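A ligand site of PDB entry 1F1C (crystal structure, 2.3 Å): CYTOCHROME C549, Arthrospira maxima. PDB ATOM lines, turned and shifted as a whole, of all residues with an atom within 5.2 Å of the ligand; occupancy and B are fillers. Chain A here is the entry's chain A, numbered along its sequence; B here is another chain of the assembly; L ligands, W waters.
The side-chain sulfur (SG) of Cys 38 is bonded to a carbon (C25) of the ligand (1.9 Å). A carbon (C18) of the ligand is covalently linked to the side-chain sulfur (SG) of Cys 35 (2.0 Å). NE2 of His 39 is bound to FE1 of the ligand (2.2 Å). A ring nitrogen (NE2) of His 90 is bound to an iron atom (FE1) of the ligand (2.2 Å). An oxygen (O4) of the ligand lies close to the side-chain carboxylate (OE1) of Glu 88 of chain B. O of Asn 51 lies close to O2 of the ligand, 2.5 Å away. The backbone NH of Tyr 80 sits at hydrogen-bond distance from an oxygen (O3) of the ligand (2.9 Å).
The side-chain hydroxyl (OG1) of Thr 44 sits close to a ring nitrogen (ND1) of His 39 (3.2 Å). The backbone carbonyl oxygen of Glu 88 of chain B sits at hydrogen-bond distance from the side-chain hydroxyl of Thr 46. The side-chain carboxylate of Glu 88 of chain B sits at hydrogen-bond distance from the side-chain amide nitrogen of Asn 47 (2.6 Å). The side-chain hydroxyl of Tyr 80 is in hydrogen-bond range of the backbone NH of Ala 60, at 3.4 Å. O of Ala 56 is in hydrogen-bond range of OH of Tyr 80. OH of Tyr 73 sits close to O of Thr 78 (3.4 Å). The side-chain hydroxyl of Thr 44 sits at hydrogen-bond distance from the backbone carbonyl oxygen of Val 50. N of Val 50 sits close to OD1 of Asn 47 (3.5 Å).
Water W2 lies within hydrogen-bond range of O3 of the ligand (2.5 Å), O of Thr 78 (3.0 Å), OH of Tyr 73 (3.0 Å) and N of Tyr 80 (3.3 Å).
Merely in contact with the ligand: Gln 37, Tyr 73, Ala 34, Val 50, Thr 46, Ala 60, Thr 79, Thr 44, Pro 91, Leu 52, Ile 86, Leu 70, Ile 74, Ile 117, Ala 56, Asn 47, Leu 57, Leu 89 of chain B, Val 113 and Met 102. Hydrophobic or aromatic side chains within 4 Å of the ligand: His 39, Val 50, Leu 52, Ala 56, Leu 57, Ala 60, Leu 70, Tyr 73, Ile 74, Tyr 80, Ile 86, His 90, Pro 91, Met 102, Val 113, Ile 117 and Leu 89 of chain B. 27 residues have an atom within 4 Å of the ligand: Ala 34, Cys 35, Gln 37, Cys 38, His 39, Thr 44, Thr 46, Asn 47, Val 50, Asn 51, Leu 52, Ala 56, Leu 57, Ala 60, Leu 70, Tyr 73, Ile 74, Thr 79, Tyr 80, Ile 86, His 90, Pro 91, Met 102, Val 113, Ile 117, Glu 88 of chain B and Leu 89 of chain B. The nearest printed residue that does not touch the ligand is Arg 64 (4.2 Å).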
ATOM      1  N   PHE A  31     -27.587   1.949  17.941  1.00  0.00           N
ATOM      2  CA  PHE A  31     -27.596   1.257  16.673  1.00  0.00           C
ATOM      3  C   PHE A  31     -28.609   1.860  15.712  1.00  0.00           C
ATOM      4  O   PHE A  31     -28.276   2.216  14.584  1.00  0.00           O
ATOM      5  CB  PHE A  31     -27.865  -0.233  16.869  1.00  0.00           C
ATOM      6  CG  PHE A  31     -27.754  -1.044  15.615  1.00  0.00           C
ATOM      7  CD1 PHE A  31     -28.833  -1.153  14.741  1.00  0.00           C
ATOM      8  CD2 PHE A  31     -26.559  -1.684  15.284  1.00  0.00           C
ATOM      9  CE1 PHE A  31     -28.729  -1.872  13.544  1.00  0.00           C
ATOM     10  CE2 PHE A  31     -26.436  -2.406  14.102  1.00  0.00           C
ATOM     11  CZ  PHE A  31     -27.517  -2.505  13.227  1.00  0.00           C
ATOM     12  N   ALA A  34     -27.224   5.315  14.613  1.00  0.00           N
ATOM     13  CA  ALA A  34     -25.985   5.407  13.817  1.00  0.00           C
ATOM     14  C   ALA A  34     -25.667   4.261  12.879  1.00  0.00           C
ATOM     15  O   ALA A  34     -24.707   4.352  12.103  1.00  0.00           O
ATOM     16  CB  ALA A  34     -24.796   5.613  14.763  1.00  0.00           C
ATOM     17  N   CYS A  35     -26.455   3.204  12.901  1.00  0.00           N
ATOM     18  CA  CYS A  35     -26.133   2.075  12.047  1.00  0.00           C
ATOM     19  C   CYS A  35     -27.232   1.553  11.148  1.00  0.00           C
ATOM     20  O   CYS A  35     -26.961   0.986  10.084  1.00  0.00           O
ATOM     21  CB  CYS A  35     -25.630   0.942  12.945  1.00  0.00           C
ATOM     22  SG  CYS A  35     -24.667   1.599  14.327  1.00  0.00           S
ATOM     23  N   GLN A  37     -29.020   2.813   9.085  1.00  0.00           N
ATOM     24  CA  GLN A  37     -29.022   3.361   7.736  1.00  0.00           C
ATOM     25  C   GLN A  37     -28.493   2.356   6.714  1.00  0.00           C
ATOM     26  O   GLN A  37     -28.986   2.269   5.603  1.00  0.00           O
ATOM     27  CB  GLN A  37     -28.170   4.622   7.688  1.00  0.00           C
ATOM     28  CG  GLN A  37     -27.928   5.169   6.289  1.00  0.00           C
ATOM     29  CD  GLN A  37     -26.807   6.181   6.282  1.00  0.00           C
ATOM     30  OE1 GLN A  37     -26.820   7.149   7.047  1.00  0.00           O
ATOM     31  NE2 GLN A  37     -25.820   5.972   5.419  1.00  0.00           N
ATOM     32  N   CYS A  38     -27.471   1.608   7.105  1.00  0.00           N
ATOM     33  CA  CYS A  38     -26.892   0.634   6.198  1.00  0.00           C
ATOM     34  C   CYS A  38     -26.934  -0.768   6.788  1.00  0.00           C
ATOM     35  O   CYS A  38     -26.542  -1.746   6.121  1.00  0.00           O
ATOM     36  CB  CYS A  38     -25.445   1.005   5.899  1.00  0.00           C
ATOM     37  SG  CYS A  38     -25.170   2.764   5.471  1.00  0.00           S
ATOM     38  N   HIS A  39     -27.411  -0.885   8.025  1.00  0.00           N
ATOM     39  CA  HIS A  39     -27.457  -2.183   8.678  1.00  0.00           C
ATOM     40  C   HIS A  39     -28.776  -2.659   9.277  1.00  0.00           C
ATOM     41  O   HIS A  39     -28.766  -3.600  10.067  1.00  0.00           O
ATOM     42  CB  HIS A  39     -26.400  -2.235   9.774  1.00  0.00           C
ATOM     43  CG  HIS A  39     -25.001  -2.203   9.262  1.00  0.00           C
ATOM     44  ND1 HIS A  39     -24.527  -3.108   8.337  1.00  0.00           N
ATOM     45  CD2 HIS A  39     -23.941  -1.427   9.615  1.00  0.00           C
ATOM     46  CE1 HIS A  39     -23.233  -2.893   8.147  1.00  0.00           C
ATOM     47  NE2 HIS A  39     -22.851  -1.888   8.910  1.00  0.00           N
ATOM     48  N   THR A  44     -26.030  -5.333   5.280  1.00  0.00           N
ATOM     49  CA  THR A  44     -25.097  -4.278   4.927  1.00  0.00           C
ATOM     50  C   THR A  44     -25.593  -3.897   3.545  1.00  0.00           C
ATOM     51  O   THR A  44     -25.319  -4.574   2.555  1.00  0.00           O
ATOM     52  CB  THR A  44     -23.642  -4.771   4.882  1.00  0.00           C
ATOM     53  OG1 THR A  44     -23.181  -5.043   6.216  1.00  0.00           O
ATOM     54  CG2 THR A  44     -22.752  -3.699   4.273  1.00  0.00           C
ATOM     55  N   THR A  46     -24.920  -1.766   1.104  1.00  0.00           N
ATOM     56  CA  THR A  46     -24.044  -1.711  -0.053  1.00  0.00           C
ATOM     57  C   THR A  46     -22.986  -2.806  -0.123  1.00  0.00           C
ATOM     58  O   THR A  46     -22.076  -2.733  -0.940  1.00  0.00           O
ATOM     59  CB  THR A  46     -23.366  -0.335  -0.136  1.00  0.00           C
ATOM     60  OG1 THR A  46     -22.712  -0.068   1.103  1.00  0.00           O
ATOM     61  CG2 THR A  46     -24.407   0.741  -0.417  1.00  0.00           C
ATOM     62  N   ASN A  47     -23.093  -3.810   0.735  1.00  0.00           N
ATOM     63  CA  ASN A  47     -22.169  -4.925   0.706  1.00  0.00           C
ATOM     64  C   ASN A  47     -22.843  -6.083   1.401  1.00  0.00           C
ATOM     65  O   ASN A  47     -22.590  -6.365   2.570  1.00  0.00           O
ATOM     66  CB  ASN A  47     -20.848  -4.612   1.409  1.00  0.00           C
ATOM     67  CG  ASN A  47     -19.779  -5.642   1.069  1.00  0.00           C
ATOM     68  OD1 ASN A  47     -20.090  -6.807   0.824  1.00  0.00           O
ATOM     69  ND2 ASN A  47     -18.529  -5.213   1.075  1.00  0.00           N
ATOM     70  N   VAL A  50     -20.699  -8.843   3.594  1.00  0.00           N
ATOM     71  CA  VAL A  50     -20.167  -8.413   4.897  1.00  0.00           C
ATOM     72  C   VAL A  50     -21.306  -7.934   5.810  1.00  0.00           C
ATOM     73  O   VAL A  50     -21.395  -6.742   6.131  1.00  0.00           O
ATOM     74  CB  VAL A  50     -19.131  -7.274   4.713  1.00  0.00           C
ATOM     75  CG1 VAL A  50     -18.354  -7.058   5.991  1.00  0.00           C
ATOM     76  CG2 VAL A  50     -18.188  -7.615   3.579  1.00  0.00           C
ATOM     77  N   ASN A  51     -22.163  -8.882   6.213  1.00  0.00           N
ATOM     78  CA  ASN A  51     -23.337  -8.650   7.061  1.00  0.00           C
ATOM     79  C   ASN A  51     -23.058  -8.565   8.568  1.00  0.00           C
ATOM     80  O   ASN A  51     -21.916  -8.577   8.998  1.00  0.00           O
ATOM     81  CB  ASN A  51     -24.340  -9.785   6.837  1.00  0.00           C
ATOM     82  CG  ASN A  51     -25.558  -9.344   6.065  1.00  0.00           C
ATOM     83  OD1 ASN A  51     -25.448  -8.790   4.957  1.00  0.00           O
ATOM     84  ND2 ASN A  51     -26.730  -9.599   6.629  1.00  0.00           N
ATOM     85  N   LEU A  52     -24.141  -8.502   9.356  1.00  0.00           N
ATOM     86  CA  LEU A  52     -24.026  -8.459  10.810  1.00  0.00           C
ATOM     87  C   LEU A  52     -24.494  -9.785  11.383  1.00  0.00           C
ATOM     88  O   LEU A  52     -24.845  -9.886  12.562  1.00  0.00           O
ATOM     89  CB  LEU A  52     -24.844  -7.310  11.412  1.00  0.00           C
ATOM     90  CG  LEU A  52     -24.316  -5.899  11.182  1.00  0.00           C
ATOM     91  CD1 LEU A  52     -25.069  -4.900  12.078  1.00  0.00           C
ATOM     92  CD2 LEU A  52     -22.826  -5.853  11.492  1.00  0.00           C
ATOM     93  N   ALA A  56     -21.000 -14.196   9.119  1.00  0.00           N
ATOM     94  CA  ALA A  56     -20.181 -13.174   8.487  1.00  0.00           C
ATOM     95  C   ALA A  56     -19.181 -12.582   9.477  1.00  0.00           C
ATOM     96  O   ALA A  56     -17.987 -12.468   9.189  1.00  0.00           O
ATOM     97  CB  ALA A  56     -21.060 -12.071   7.894  1.00  0.00           C
ATOM     98  N   LEU A  57     -19.674 -12.215  10.657  1.00  0.00           N
ATOM     99  CA  LEU A  57     -18.826 -11.645  11.697  1.00  0.00           C
ATOM    100  C   LEU A  57     -17.678 -12.582  12.050  1.00  0.00           C
ATOM    101  O   LEU A  57     -16.533 -12.165  12.161  1.00  0.00           O
ATOM    102  CB  LEU A  57     -19.660 -11.362  12.957  1.00  0.00           C
ATOM    103  CG  LEU A  57     -20.675 -10.216  12.916  1.00  0.00           C
ATOM    104  CD1 LEU A  57     -21.450 -10.139  14.229  1.00  0.00           C
ATOM    105  CD2 LEU A  57     -19.922  -8.919  12.665  1.00  0.00           C
ATOM    106  N   ALA A  60     -14.830 -12.626   9.552  1.00  0.00           N
ATOM    107  CA  ALA A  60     -14.142 -11.364   9.294  1.00  0.00           C
ATOM    108  C   ALA A  60     -12.709 -11.491   9.798  1.00  0.00           C
ATOM    109  O   ALA A  60     -12.343 -12.481  10.436  1.00  0.00           O
ATOM    110  CB  ALA A  60     -14.857 -10.223  10.022  1.00  0.00           C
ATOM    111  N   ARG A  64     -15.177 -10.619  14.231  1.00  0.00           N
ATOM    112  CA  ARG A  64     -15.871  -9.550  14.937  1.00  0.00           C
ATOM    113  C   ARG A  64     -17.028 -10.169  15.706  1.00  0.00           C
ATOM    114  O   ARG A  64     -18.079  -9.542  15.866  1.00  0.00           O
ATOM    115  CB  ARG A  64     -16.390  -8.524  13.928  1.00  0.00           C
ATOM    116  CG  ARG A  64     -15.294  -7.928  13.046  1.00  0.00           C
ATOM    117  CD  ARG A  64     -14.276  -7.164  13.880  1.00  0.00           C
ATOM    118  NE  ARG A  64     -13.302  -6.448  13.051  1.00  0.00           N
ATOM    119  CZ  ARG A  64     -12.472  -5.521  13.519  1.00  0.00           C
ATOM    120  NH1 ARG A  64     -12.489  -5.193  14.807  1.00  0.00           N
ATOM    121  NH2 ARG A  64     -11.625  -4.921  12.698  1.00  0.00           N
ATOM    122  N   LEU A  70     -16.018  -6.129  18.292  1.00  0.00           N
ATOM    123  CA  LEU A  70     -17.012  -5.229  17.736  1.00  0.00           C
ATOM    124  C   LEU A  70     -16.716  -3.791  18.183  1.00  0.00           C
ATOM    125  O   LEU A  70     -16.817  -2.850  17.387  1.00  0.00           O
ATOM    126  CB  LEU A  70     -18.412  -5.648  18.174  1.00  0.00           C
ATOM    127  CG  LEU A  70     -18.905  -6.891  17.422  1.00  0.00           C
ATOM    128  CD1 LEU A  70     -20.278  -7.293  17.923  1.00  0.00           C
ATOM    129  CD2 LEU A  70     -18.939  -6.586  15.917  1.00  0.00           C
ATOM    130  N   TYR A  73     -13.881  -2.481  16.187  1.00  0.00           N
ATOM    131  CA  TYR A  73     -14.339  -2.179  14.843  1.00  0.00           C
ATOM    132  C   TYR A  73     -14.908  -0.774  14.707  1.00  0.00           C
ATOM    133  O   TYR A  73     -14.574  -0.062  13.763  1.00  0.00           O
ATOM    134  CB  TYR A  73     -15.403  -3.190  14.399  1.00  0.00           C
ATOM    135  CG  TYR A  73     -15.720  -3.025  12.942  1.00  0.00           C
ATOM    136  CD1 TYR A  73     -14.959  -3.676  11.959  1.00  0.00           C
ATOM    137  CD2 TYR A  73     -16.714  -2.141  12.525  1.00  0.00           C
ATOM    138  CE1 TYR A  73     -15.171  -3.440  10.605  1.00  0.00           C
ATOM    139  CE2 TYR A  73     -16.925  -1.884  11.176  1.00  0.00           C
ATOM    140  CZ  TYR A  73     -16.164  -2.540  10.217  1.00  0.00           C
ATOM    141  OH  TYR A  73     -16.391  -2.294   8.879  1.00  0.00           O
ATOM    142  N   ILE A  74     -15.774  -0.382  15.637  1.00  0.00           N
ATOM    143  CA  ILE A  74     -16.366   0.949  15.576  1.00  0.00           C
ATOM    144  C   ILE A  74     -15.327   2.015  15.837  1.00  0.00           C
ATOM    145  O   ILE A  74     -15.371   3.100  15.247  1.00  0.00           O
ATOM    146  CB  ILE A  74     -17.508   1.094  16.592  1.00  0.00           C
ATOM    147  CG1 ILE A  74     -18.566   0.032  16.316  1.00  0.00           C
ATOM    148  CG2 ILE A  74     -18.101   2.502  16.499  1.00  0.00           C
ATOM    149  CD1 ILE A  74     -19.575  -0.150  17.441  1.00  0.00           C
ATOM    150  N   THR A  78     -12.305  -1.411   9.546  1.00  0.00           N
ATOM    151  CA  THR A  78     -11.413  -1.940   8.518  1.00  0.00           C
ATOM    152  C   THR A  78     -12.211  -2.828   7.555  1.00  0.00           C
ATOM    153  O   THR A  78     -13.267  -3.356   7.919  1.00  0.00           O
ATOM    154  CB  THR A  78     -10.295  -2.807   9.113  1.00  0.00           C
ATOM    155  OG1 THR A  78     -10.856  -4.057   9.526  1.00  0.00           O
ATOM    156  CG2 THR A  78      -9.639  -2.116  10.292  1.00  0.00           C
ATOM    157  N   THR A  79     -11.708  -2.995   6.327  1.00  0.00           N
ATOM    158  CA  THR A  79     -12.397  -3.833   5.349  1.00  0.00           C
ATOM    159  C   THR A  79     -12.616  -5.212   5.919  1.00  0.00           C
ATOM    160  O   THR A  79     -12.054  -5.562   6.950  1.00  0.00           O
ATOM    161  CB  THR A  79     -11.593  -3.965   4.038  1.00  0.00           C
ATOM    162  OG1 THR A  79     -10.203  -4.187   4.351  1.00  0.00           O
ATOM    163  CG2 THR A  79     -11.730  -2.707   3.194  1.00  0.00           C
ATOM    164  N   TYR A  80     -13.421  -6.016   5.250  1.00  0.00           N
ATOM    165  CA  TYR A  80     -13.691  -7.358   5.743  1.00  0.00           C
ATOM    166  C   TYR A  80     -12.405  -8.149   5.952  1.00  0.00           C
ATOM    167  O   TYR A  80     -12.246  -8.843   6.959  1.00  0.00           O
ATOM    168  CB  TYR A  80     -14.607  -8.094   4.778  1.00  0.00           C
ATOM    169  CG  TYR A  80     -15.203  -9.351   5.354  1.00  0.00           C
ATOM    170  CD1 TYR A  80     -15.974  -9.300   6.527  1.00  0.00           C
ATOM    171  CD2 TYR A  80     -15.030 -10.583   4.727  1.00  0.00           C
ATOM    172  CE1 TYR A  80     -16.563 -10.452   7.049  1.00  0.00           C
ATOM    173  CE2 TYR A  80     -15.623 -11.737   5.241  1.00  0.00           C
ATOM    174  CZ  TYR A  80     -16.379 -11.664   6.401  1.00  0.00           C
ATOM    175  OH  TYR A  80     -16.960 -12.809   6.896  1.00  0.00           O
ATOM    176  N   ILE A  86     -10.968   1.813   6.970  1.00  0.00           N
ATOM    177  CA  ILE A  86     -12.008   2.575   6.280  1.00  0.00           C
ATOM    178  C   ILE A  86     -12.745   3.540   7.201  1.00  0.00           C
ATOM    179  O   ILE A  86     -13.932   3.804   7.002  1.00  0.00           O
ATOM    180  CB  ILE A  86     -13.028   1.624   5.609  1.00  0.00           C
ATOM    181  CG1 ILE A  86     -13.649   0.696   6.646  1.00  0.00           C
ATOM    182  CG2 ILE A  86     -12.344   0.779   4.556  1.00  0.00           C
ATOM    183  CD1 ILE A  86     -14.668  -0.251   6.053  1.00  0.00           C
ATOM    184  N   HIS A  90     -16.273   5.014   6.842  1.00  0.00           N
ATOM    185  CA  HIS A  90     -17.206   4.255   7.676  1.00  0.00           C
ATOM    186  C   HIS A  90     -17.328   4.906   9.034  1.00  0.00           C
ATOM    187  O   HIS A  90     -16.340   5.384   9.589  1.00  0.00           O
ATOM    188  CB  HIS A  90     -16.756   2.803   7.854  1.00  0.00           C
ATOM    189  CG  HIS A  90     -17.722   1.941   8.618  1.00  0.00           C
ATOM    190  ND1 HIS A  90     -17.898   2.055   9.988  1.00  0.00           N
ATOM    191  CD2 HIS A  90     -18.581   0.969   8.220  1.00  0.00           C
ATOM    192  CE1 HIS A  90     -18.806   1.180  10.393  1.00  0.00           C
ATOM    193  NE2 HIS A  90     -19.239   0.504   9.338  1.00  0.00           N
ATOM    194  N   PRO A  91     -18.548   4.951   9.594  1.00  0.00           N
ATOM    195  CA  PRO A  91     -18.766   5.564  10.902  1.00  0.00           C
ATOM    196  C   PRO A  91     -17.769   5.055  11.946  1.00  0.00           C
ATOM    197  O   PRO A  91     -17.522   3.862  12.062  1.00  0.00           O
ATOM    198  CB  PRO A  91     -20.206   5.176  11.214  1.00  0.00           C
ATOM    199  CG  PRO A  91     -20.852   5.263   9.865  1.00  0.00           C
ATOM    200  CD  PRO A  91     -19.834   4.550   8.990  1.00  0.00           C
ATOM    201  N   PHE A  99     -20.316  11.974  10.089  1.00  0.00           N
ATOM    202  CA  PHE A  99     -21.274  11.131  10.776  1.00  0.00           C
ATOM    203  C   PHE A  99     -21.589  11.744  12.138  1.00  0.00           C
ATOM    204  O   PHE A  99     -21.099  11.278  13.176  1.00  0.00           O
ATOM    205  CB  PHE A  99     -20.704   9.720  10.936  1.00  0.00           C
ATOM    206  CG  PHE A  99     -20.435   9.035   9.625  1.00  0.00           C
ATOM    207  CD1 PHE A  99     -21.469   8.777   8.739  1.00  0.00           C
ATOM    208  CD2 PHE A  99     -19.144   8.661   9.281  1.00  0.00           C
ATOM    209  CE1 PHE A  99     -21.226   8.163   7.509  1.00  0.00           C
ATOM    210  CE2 PHE A  99     -18.885   8.041   8.058  1.00  0.00           C
ATOM    211  CZ  PHE A  99     -19.931   7.792   7.174  1.00  0.00           C
ATOM    212  N   MET A 102     -21.860  10.174  15.657  1.00  0.00           N
ATOM    213  CA  MET A 102     -20.706   9.549  16.294  1.00  0.00           C
ATOM    214  C   MET A 102     -19.940  10.532  17.189  1.00  0.00           C
ATOM    215  O   MET A 102     -18.904  10.182  17.757  1.00  0.00           O
ATOM    216  CB  MET A 102     -19.749   8.996  15.233  1.00  0.00           C
ATOM    217  CG  MET A 102     -20.347   7.930  14.322  1.00  0.00           C
ATOM    218  SD  MET A 102     -20.987   6.494  15.213  1.00  0.00           S
ATOM    219  CE  MET A 102     -19.448   5.773  15.867  1.00  0.00           C
ATOM    220  N   VAL A 113     -23.839  -1.373  21.973  1.00  0.00           N
ATOM    221  CA  VAL A 113     -24.178  -1.665  20.594  1.00  0.00           C
ATOM    222  C   VAL A 113     -23.634  -3.049  20.252  1.00  0.00           C
ATOM    223  O   VAL A 113     -24.293  -3.820  19.545  1.00  0.00           O
ATOM    224  CB  VAL A 113     -23.576  -0.614  19.621  1.00  0.00           C
ATOM    225  CG1 VAL A 113     -24.083  -0.864  18.202  1.00  0.00           C
ATOM    226  CG2 VAL A 113     -23.964   0.778  20.062  1.00  0.00           C
ATOM    227  N   ILE A 117     -25.904  -6.024  18.796  1.00  0.00           N
ATOM    228  CA  ILE A 117     -25.616  -6.715  17.546  1.00  0.00           C
ATOM    229  C   ILE A 117     -25.531  -8.224  17.762  1.00  0.00           C
ATOM    230  O   ILE A 117     -26.160  -8.984  17.027  1.00  0.00           O
ATOM    231  CB  ILE A 117     -24.282  -6.222  16.914  1.00  0.00           C
ATOM    232  CG1 ILE A 117     -24.453  -4.775  16.404  1.00  0.00           C
ATOM    233  CG2 ILE A 117     -23.860  -7.184  15.792  1.00  0.00           C
ATOM    234  CD1 ILE A 117     -23.164  -4.112  15.835  1.00  0.00           C
ATOM    235  N   GLU B  88     -18.920   0.856  -2.178  1.00  0.00           N
ATOM    236  CA  GLU B  88     -19.899   0.539  -1.142  1.00  0.00           C
ATOM    237  C   GLU B  88     -20.028   1.685  -0.129  1.00  0.00           C
ATOM    238  O   GLU B  88     -21.071   1.863   0.509  1.00  0.00           O
ATOM    239  CB  GLU B  88     -19.448  -0.702  -0.382  1.00  0.00           C
ATOM    240  CG  GLU B  88     -18.125  -0.470   0.331  1.00  0.00           C
ATOM    241  CD  GLU B  88     -17.724  -1.598   1.250  1.00  0.00           C
ATOM    242  OE1 GLU B  88     -16.704  -1.448   1.958  1.00  0.00           O
ATOM    243  OE2 GLU B  88     -18.426  -2.633   1.295  1.00  0.00           O
ATOM    244  N   LEU B  89     -18.947   2.450   0.027  1.00  0.00           N
ATOM    245  CA  LEU B  89     -18.908   3.546   0.981  1.00  0.00           C
ATOM    246  C   LEU B  89     -18.657   4.906   0.380  1.00  0.00           C
ATOM    247  O   LEU B  89     -18.836   5.918   1.058  1.00  0.00           O
ATOM    248  CB  LEU B  89     -17.836   3.271   2.030  1.00  0.00           C
ATOM    249  CG  LEU B  89     -18.263   2.286   3.111  1.00  0.00           C
ATOM    250  CD1 LEU B  89     -17.070   1.870   3.932  1.00  0.00           C
ATOM    251  CD2 LEU B  89     -19.350   2.935   3.988  1.00  0.00           C
ATOM    252  N   ILE B  98     -27.243   4.788  -0.673  1.00  0.00           N
ATOM    253  CA  ILE B  98     -26.942   5.630   0.473  1.00  0.00           C
ATOM    254  C   ILE B  98     -26.517   7.036   0.042  1.00  0.00           C
ATOM    255  O   ILE B  98     -26.157   7.871   0.861  1.00  0.00           O
ATOM    256  CB  ILE B  98     -25.843   4.997   1.349  1.00  0.00           C
ATOM    257  CG1 ILE B  98     -24.582   4.722   0.508  1.00  0.00           C
ATOM    258  CG2 ILE B  98     -26.352   3.675   1.928  1.00  0.00           C
ATOM    259  CD1 ILE B  98     -23.492   3.994   1.268  1.00  0.00           C
HETATM  260 FE1  LIG L   1     -21.101  -0.631   9.149  1.00  0.00          FE
HETATM  261  C1  LIG L   1     -19.273  -3.219   7.905  1.00  0.00           C
HETATM  262  C2  LIG L   1     -20.980  -2.115  12.317  1.00  0.00           C
HETATM  263  C3  LIG L   1     -22.742   2.002  10.545  1.00  0.00           C
HETATM  264  C4  LIG L   1     -21.641   0.550   6.030  1.00  0.00           C
HETATM  265  N1  LIG L   1     -20.249  -2.252   9.939  1.00  0.00           N
HETATM  266  C5  LIG L   1     -19.521  -3.201   9.288  1.00  0.00           C
HETATM  267  C6  LIG L   1     -19.154  -4.254  10.201  1.00  0.00           C
HETATM  268  C7  LIG L   1     -19.626  -3.949  11.411  1.00  0.00           C
HETATM  269  C8  LIG L   1     -20.342  -2.735  11.244  1.00  0.00           C
HETATM  270  C9  LIG L   1     -19.298  -4.612  12.741  1.00  0.00           C
HETATM  271  C10 LIG L   1     -18.356  -5.471   9.872  1.00  0.00           C
HETATM  272  C11 LIG L   1     -19.329  -6.497   9.359  1.00  0.00           C
HETATM  273  C12 LIG L   1     -18.684  -7.838   9.198  1.00  0.00           C
HETATM  274  O1  LIG L   1     -17.463  -7.936   9.415  1.00  0.00           O
HETATM  275  O2  LIG L   1     -19.390  -8.802   8.844  1.00  0.00           O
HETATM  276  N2  LIG L   1     -21.694  -0.149  11.003  1.00  0.00           N
HETATM  277  C13 LIG L   1     -21.589  -0.893  12.192  1.00  0.00           C
HETATM  278  C14 LIG L   1     -22.070  -0.158  13.323  1.00  0.00           C
HETATM  279  C15 LIG L   1     -22.439   1.049  12.851  1.00  0.00           C
HETATM  280  C16 LIG L   1     -22.272   1.034  11.414  1.00  0.00           C
HETATM  281  C17 LIG L   1     -22.178  -0.629  14.766  1.00  0.00           C
HETATM  282  C18 LIG L   1     -22.866   2.123  13.631  1.00  0.00           C
HETATM  283  C19 LIG L   1     -22.019   2.728  14.583  1.00  0.00           C
HETATM  284  N3  LIG L   1     -22.021   0.907   8.432  1.00  0.00           N
HETATM  285  C20 LIG L   1     -22.667   1.895   9.150  1.00  0.00           C
HETATM  286  C21 LIG L   1     -23.239   2.873   8.278  1.00  0.00           C
HETATM  287  C22 LIG L   1     -22.889   2.522   7.010  1.00  0.00           C
HETATM  288  C23 LIG L   1     -22.165   1.255   7.108  1.00  0.00           C
HETATM  289  C24 LIG L   1     -24.139   4.042   8.686  1.00  0.00           C
HETATM  290  C25 LIG L   1     -23.324   3.202   5.834  1.00  0.00           C
HETATM  291  C26 LIG L   1     -22.993   4.573   5.599  1.00  0.00           C
HETATM  292  N4  LIG L   1     -20.520  -1.178   7.351  1.00  0.00           N
HETATM  293  C27 LIG L   1     -20.792  -0.552   6.153  1.00  0.00           C
HETATM  294  C28 LIG L   1     -20.176  -1.220   5.069  1.00  0.00           C
HETATM  295  C29 LIG L   1     -19.513  -2.264   5.594  1.00  0.00           C
HETATM  296  C30 LIG L   1     -19.753  -2.268   7.012  1.00  0.00           C
HETATM  297  C31 LIG L   1     -20.420  -0.936   3.559  1.00  0.00           C
HETATM  298  C32 LIG L   1     -18.603  -3.245   4.850  1.00  0.00           C
HETATM  299  C33 LIG L   1     -17.160  -2.743   4.764  1.00  0.00           C
HETATM  300  C34 LIG L   1     -16.221  -3.744   4.102  1.00  0.00           C
HETATM  301  O3  LIG L   1     -15.967  -4.822   4.667  1.00  0.00           O
HETATM  302  O4  LIG L   1     -15.731  -3.458   2.982  1.00  0.00           O
HETATM  303  O   HOH W   1     -14.887  -6.918   8.868  1.00  0.00           O
HETATM  304  O   HOH W   2     -15.816  -4.757   7.211  1.00  0.00           O
